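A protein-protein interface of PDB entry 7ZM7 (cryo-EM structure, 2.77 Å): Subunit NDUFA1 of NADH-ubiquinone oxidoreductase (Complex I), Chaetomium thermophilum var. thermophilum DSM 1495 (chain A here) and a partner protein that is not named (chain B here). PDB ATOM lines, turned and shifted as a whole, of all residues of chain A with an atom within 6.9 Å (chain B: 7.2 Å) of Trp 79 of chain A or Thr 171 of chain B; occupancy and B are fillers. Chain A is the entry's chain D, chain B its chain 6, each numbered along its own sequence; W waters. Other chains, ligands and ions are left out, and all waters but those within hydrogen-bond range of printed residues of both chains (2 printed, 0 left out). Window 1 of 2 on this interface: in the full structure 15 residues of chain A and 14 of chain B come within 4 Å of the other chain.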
ATOM      1  N   ASN A  76     -16.965 -11.748 -16.410  1.00  0.00           N
ATOM      2  CA  ASN A  76     -17.733 -12.525 -17.422  1.00  0.00           C
ATOM      3  C   ASN A  76     -18.559 -11.599 -18.310  1.00  0.00           C
ATOM      4  O   ASN A  76     -19.295 -12.123 -19.157  1.00  0.00           O
ATOM      5  CB  ASN A  76     -18.538 -13.673 -16.810  1.00  0.00           C
ATOM      6  CG  ASN A  76     -19.597 -13.275 -15.807  1.00  0.00           C
ATOM      7  OD1 ASN A  76     -20.037 -12.135 -15.772  1.00  0.00           O
ATOM      8  ND2 ASN A  76     -20.034 -14.227 -15.002  1.00  0.00           N
ATOM      9  N   ASN A  77     -18.422 -10.286 -18.129  1.00  0.00           N
ATOM     10  CA  ASN A  77     -19.162  -9.275 -18.929  1.00  0.00           C
ATOM     11  C   ASN A  77     -18.753  -9.473 -20.381  1.00  0.00           C
ATOM     12  O   ASN A  77     -17.567  -9.284 -20.674  1.00  0.00           O
ATOM     13  CB  ASN A  77     -18.915  -7.852 -18.428  1.00  0.00           C
ATOM     14  CG  ASN A  77     -19.755  -6.823 -19.152  1.00  0.00           C
ATOM     15  OD1 ASN A  77     -20.896  -7.092 -19.515  1.00  0.00           O
ATOM     16  ND2 ASN A  77     -19.203  -5.641 -19.364  1.00  0.00           N
ATOM     17  N   PRO A  78     -19.669  -9.793 -21.309  1.00  0.00           N
ATOM     18  CA  PRO A  78     -19.276 -10.124 -22.674  1.00  0.00           C
ATOM     19  C   PRO A  78     -19.123  -8.909 -23.591  1.00  0.00           C
ATOM     20  O   PRO A  78     -20.058  -8.161 -23.732  1.00  0.00           O
ATOM     21  CB  PRO A  78     -20.426 -11.025 -23.133  1.00  0.00           C
ATOM     22  CG  PRO A  78     -21.636 -10.589 -22.323  1.00  0.00           C
ATOM     23  CD  PRO A  78     -21.114  -9.854 -21.105  1.00  0.00           C
ATOM     24  N   TRP A  79     -17.929  -8.691 -24.138  1.00  0.00           N
ATOM     25  CA  TRP A  79     -17.772  -7.613 -25.147  1.00  0.00           C
ATOM     26  C   TRP A  79     -17.751  -8.301 -26.507  1.00  0.00           C
ATOM     27  O   TRP A  79     -16.825  -9.072 -26.758  1.00  0.00           O
ATOM     28  CB  TRP A  79     -16.526  -6.755 -24.897  1.00  0.00           C
ATOM     29  CG  TRP A  79     -16.630  -5.757 -23.786  1.00  0.00           C
ATOM     30  CD1 TRP A  79     -17.538  -5.739 -22.770  1.00  0.00           C
ATOM     31  CD2 TRP A  79     -15.766  -4.627 -23.571  1.00  0.00           C
ATOM     32  NE1 TRP A  79     -17.305  -4.673 -21.945  1.00  0.00           N
ATOM     33  CE2 TRP A  79     -16.224  -3.974 -22.410  1.00  0.00           C
ATOM     34  CE3 TRP A  79     -14.652  -4.108 -24.239  1.00  0.00           C
ATOM     35  CZ2 TRP A  79     -15.612  -2.826 -21.911  1.00  0.00           C
ATOM     36  CZ3 TRP A  79     -14.045  -2.976 -23.744  1.00  0.00           C
ATOM     37  CH2 TRP A  79     -14.522  -2.344 -22.597  1.00  0.00           C
ATOM     38  N   LYS A  80     -18.736  -8.020 -27.347  1.00  0.00           N
ATOM     39  CA  LYS A  80     -18.864  -8.698 -28.657  1.00  0.00           C
ATOM     40  C   LYS A  80     -17.822  -8.198 -29.661  1.00  0.00           C
ATOM     41  O   LYS A  80     -17.471  -7.017 -29.626  1.00  0.00           O
ATOM     42  CB  LYS A  80     -20.316  -8.593 -29.123  1.00  0.00           C
ATOM     43  CG  LYS A  80     -21.315  -9.284 -28.209  1.00  0.00           C
ATOM     44  CD  LYS A  80     -22.742  -8.885 -28.479  1.00  0.00           C
ATOM     45  CE  LYS A  80     -23.738  -9.906 -27.975  1.00  0.00           C
ATOM     46  NZ  LYS A  80     -25.102  -9.626 -28.478  1.00  0.00           N
ATOM     47  N   VAL A  81     -17.317  -9.051 -30.502  1.00  0.00           N
ATOM     48  CA  VAL A  81     -16.293  -8.667 -31.513  1.00  0.00           C
ATOM     49  C   VAL A  81     -16.818  -9.040 -32.896  1.00  0.00           C
ATOM     50  O   VAL A  81     -17.461 -10.099 -33.022  1.00  0.00           O
ATOM     51  CB  VAL A  81     -14.897  -9.258 -31.222  1.00  0.00           C
ATOM     52  CG1 VAL A  81     -14.540  -9.224 -29.751  1.00  0.00           C
ATOM     53  CG2 VAL A  81     -14.719 -10.662 -31.771  1.00  0.00           C
ATOM     54  N   UNK A  82     -16.607  -8.200 -33.873  1.00  0.00           N
ATOM     55  CA  UNK A  82     -17.077  -8.380 -35.231  1.00  0.00           C
ATOM     56  C   UNK A  82     -15.932  -8.097 -36.181  1.00  0.00           C
ATOM     57  O   UNK A  82     -14.973  -7.404 -35.843  1.00  0.00           O
ATOM     58  CB  UNK A  82     -18.262  -7.460 -35.552  1.00  0.00           C
ATOM     59  N   UNK A  85     -19.066  -5.080 -39.819  1.00  0.00           N
ATOM     60  CA  UNK A  85     -19.980  -3.949 -39.793  1.00  0.00           C
ATOM     61  C   UNK A  85     -19.791  -3.120 -38.536  1.00  0.00           C
ATOM     62  O   UNK A  85     -19.401  -3.624 -37.484  1.00  0.00           O
ATOM     63  CB  UNK A  85     -21.432  -4.392 -39.910  1.00  0.00           C
ATOM     64  N   LEU B   8      -9.248 -13.270 -23.568  1.00  0.00           N
ATOM     65  CA  LEU B   8      -9.861 -14.589 -23.863  1.00  0.00           C
ATOM     66  C   LEU B   8     -10.872 -14.467 -25.007  1.00  0.00           C
ATOM     67  O   LEU B   8     -11.763 -13.624 -24.908  1.00  0.00           O
ATOM     68  CB  LEU B   8     -10.510 -15.113 -22.582  1.00  0.00           C
ATOM     69  CG  LEU B   8      -9.555 -15.737 -21.568  1.00  0.00           C
ATOM     70  CD1 LEU B   8     -10.335 -16.500 -20.512  1.00  0.00           C
ATOM     71  CD2 LEU B   8      -8.571 -16.666 -22.260  1.00  0.00           C
ATOM     72  N   LEU B   9     -10.756 -15.195 -26.053  1.00  0.00           N
ATOM     73  CA  LEU B   9     -11.675 -15.105 -27.214  1.00  0.00           C
ATOM     74  C   LEU B   9     -12.444 -16.421 -27.326  1.00  0.00           C
ATOM     75  O   LEU B   9     -11.789 -17.472 -27.411  1.00  0.00           O
ATOM     76  CB  LEU B   9     -10.831 -14.873 -28.471  1.00  0.00           C
ATOM     77  CG  LEU B   9     -11.601 -14.478 -29.729  1.00  0.00           C
ATOM     78  CD1 LEU B   9     -12.385 -13.195 -29.499  1.00  0.00           C
ATOM     79  CD2 LEU B   9     -10.651 -14.312 -30.903  1.00  0.00           C
ATOM     80  N   GLU B  12     -19.899 -17.180 -29.706  1.00  0.00           N
ATOM     81  CA  GLU B  12     -21.188 -16.839 -29.035  1.00  0.00           C
ATOM     82  C   GLU B  12     -22.206 -17.942 -29.346  1.00  0.00           C
ATOM     83  O   GLU B  12     -22.488 -18.155 -30.540  1.00  0.00           O
ATOM     84  CB  GLU B  12     -21.724 -15.499 -29.533  1.00  0.00           C
ATOM     85  CG  GLU B  12     -20.733 -14.358 -29.412  1.00  0.00           C
ATOM     86  CD  GLU B  12     -21.203 -13.066 -30.059  1.00  0.00           C
ATOM     87  OE1 GLU B  12     -22.237 -13.095 -30.741  1.00  0.00           O
ATOM     88  OE2 GLU B  12     -20.535 -12.038 -29.874  1.00  0.00           O
ATOM     89  N   PHE B 169     -13.659  -5.097 -34.662  1.00  0.00           N
ATOM     90  CA  PHE B 169     -14.481  -4.032 -34.034  1.00  0.00           C
ATOM     91  C   PHE B 169     -15.032  -4.602 -32.728  1.00  0.00           C
ATOM     92  O   PHE B 169     -15.355  -5.792 -32.689  1.00  0.00           O
ATOM     93  CB  PHE B 169     -15.653  -3.661 -34.942  1.00  0.00           C
ATOM     94  CG  PHE B 169     -15.300  -2.766 -36.100  1.00  0.00           C
ATOM     95  CD1 PHE B 169     -15.147  -1.402 -35.916  1.00  0.00           C
ATOM     96  CD2 PHE B 169     -15.136  -3.285 -37.372  1.00  0.00           C
ATOM     97  CE1 PHE B 169     -14.833  -0.575 -36.981  1.00  0.00           C
ATOM     98  CE2 PHE B 169     -14.819  -2.458 -38.435  1.00  0.00           C
ATOM     99  CZ  PHE B 169     -14.672  -1.106 -38.237  1.00  0.00           C
ATOM    100  N   ILE B 170     -15.120  -3.779 -31.690  1.00  0.00           N
ATOM    101  CA  ILE B 170     -15.587  -4.266 -30.360  1.00  0.00           C
ATOM    102  C   ILE B 170     -16.831  -3.479 -29.953  1.00  0.00           C
ATOM    103  O   ILE B 170     -16.885  -2.279 -30.260  1.00  0.00           O
ATOM    104  CB  ILE B 170     -14.459  -4.198 -29.304  1.00  0.00           C
ATOM    105  CG1 ILE B 170     -14.848  -4.872 -27.986  1.00  0.00           C
ATOM    106  CG2 ILE B 170     -13.963  -2.776 -29.089  1.00  0.00           C
ATOM    107  CD1 ILE B 170     -14.339  -6.279 -27.846  1.00  0.00           C
ATOM    108  N   THR B 171     -17.806  -4.143 -29.330  1.00  0.00           N
ATOM    109  CA  THR B 171     -19.002  -3.429 -28.816  1.00  0.00           C
ATOM    110  C   THR B 171     -19.325  -3.865 -27.384  1.00  0.00           C
ATOM    111  O   THR B 171     -19.012  -5.010 -27.041  1.00  0.00           O
ATOM    112  CB  THR B 171     -20.219  -3.578 -29.737  1.00  0.00           C
ATOM    113  OG1 THR B 171     -20.314  -4.931 -30.182  1.00  0.00           O
ATOM    114  CG2 THR B 171     -20.185  -2.626 -30.910  1.00  0.00           C
ATOM    115  N   SER B 172     -19.938  -2.979 -26.598  1.00  0.00           N
ATOM    116  CA  SER B 172     -20.325  -3.271 -25.193  1.00  0.00           C
ATOM    117  C   SER B 172     -21.697  -2.644 -24.940  1.00  0.00           C
ATOM    118  O   SER B 172     -22.120  -1.826 -25.773  1.00  0.00           O
ATOM    119  CB  SER B 172     -19.301  -2.746 -24.238  1.00  0.00           C
ATOM    120  OG  SER B 172     -19.746  -2.860 -22.898  1.00  0.00           O
ATOM    121  N   LYS B 173     -22.368  -3.016 -23.847  1.00  0.00           N
ATOM    122  CA  LYS B 173     -23.743  -2.525 -23.567  1.00  0.00           C
ATOM    123  C   LYS B 173     -23.744  -1.165 -22.864  1.00  0.00           C
ATOM    124  O   LYS B 173     -22.697  -0.787 -22.321  1.00  0.00           O
ATOM    125  CB  LYS B 173     -24.489  -3.575 -22.738  1.00  0.00           C
ATOM    126  CG  LYS B 173     -23.816  -4.006 -21.446  1.00  0.00           C
ATOM    127  CD  LYS B 173     -24.559  -5.098 -20.711  1.00  0.00           C
ATOM    128  CE  LYS B 173     -24.643  -6.395 -21.487  1.00  0.00           C
ATOM    129  NZ  LYS B 173     -25.306  -7.459 -20.698  1.00  0.00           N
HETATM  130  O   HOH W   1     -18.956  -5.778 -32.391  1.00  0.00           O
HETATM  131  O   HOH W   2     -20.966  -5.514 -22.023  1.00  0.00           O
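Among the printed residues, pairs that only touch across the chains: Trp 79 of chain A with Ile 170 of chain B (3.7 Å), Trp 79 of chain A with Thr 171 of chain B (3.4 Å), Lys 80 of chain A with Glu 12 of chain B (3.3 Å), Lys 80 of chain A with Phe 169 of chain B (3.9 Å), Lys 80 of chain A with Ile 170 of chain B (3.4 Å), Val 81 of chain A with Phe 169 of chain B (3.2 Å) and Val 81 of chain A with Ile 170 of chain B (3.5 Å).
NE1 of Trp 79 of chain A sits close to ND2 of Asn 77 of chain A.
Of the 8 printed residues of chain B, 5 touch a printed residue of chain A. Hydrophobic or aromatic side chains of chain B within 4 Å of the printed part of chain A: Phe 169 and Ile 170. Hydrophobic or aromatic side chains of chain A that line the printed part of chain B: Trp 79 and Val 81. Among the printed residues, 10 pairs touch across the chains. Among the printed residues, no Asp or Glu carboxylate lies within 4 Å of a Lys or Arg side-chain nitrogen of the other chain.
The backbone carbonyl oxygen of Lys 80 of chain A is in hydrogen-bond range of the backbone NH of Thr 171 of chain B (2.9 Å). O of UNK 82 of chain A is in hydrogen-bond range of the backbone NH of Phe 169 of chain B (2.9 Å). OG of Ser 172 of chain B lies within hydrogen-bond range of NE1 of Trp 79 of chain A.
Trp 79 of chain A touches three residues of chain B. Of the printed residues of chain A, Glu 12 of chain B touches Lys 80 (3.3 Å). Of the printed residues of chain A, Ile 170 of chain B touches Trp 79 (3.7 Å), Lys 80 (3.4 Å) and Val 81 (3.5 Å). Of the printed residues of chain B, UNK 82 of chain A touches Phe 169. Of the printed residues of chain B, Lys 80 of chain A touches Glu 12 (3.3 Å), Phe 169 (3.9 Å), Ile 170 (3.4 Å) and Thr 171 (2.9 Å). Lys 173 of chain B touches none of the printed residues of chain A. Asn 76 of chain A touches none of the printed residues of chain B. The nearest printed residue of chain B that does not touch Lys 80 of chain A is Ser 172 of chain B (5.2 Å).
Water W1 bridges the side-chain hydroxyl of Thr 171 of chain B (2.7 Å) and the backbone carbonyl oxygen of Lys 80 of chain A (3.4 Å). Water W2 lies within hydrogen-bond range of the side-chain amide oxygen of Asn 77 of chain A (3.0 Å), the side-chain hydroxyl of Ser 172 of chain B (3.0 Å), the backbone carbonyl oxygen of Pro 78 of chain A (3.3 Å) and the backbone NH of Lys 173 of chain B (3.4 Å).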
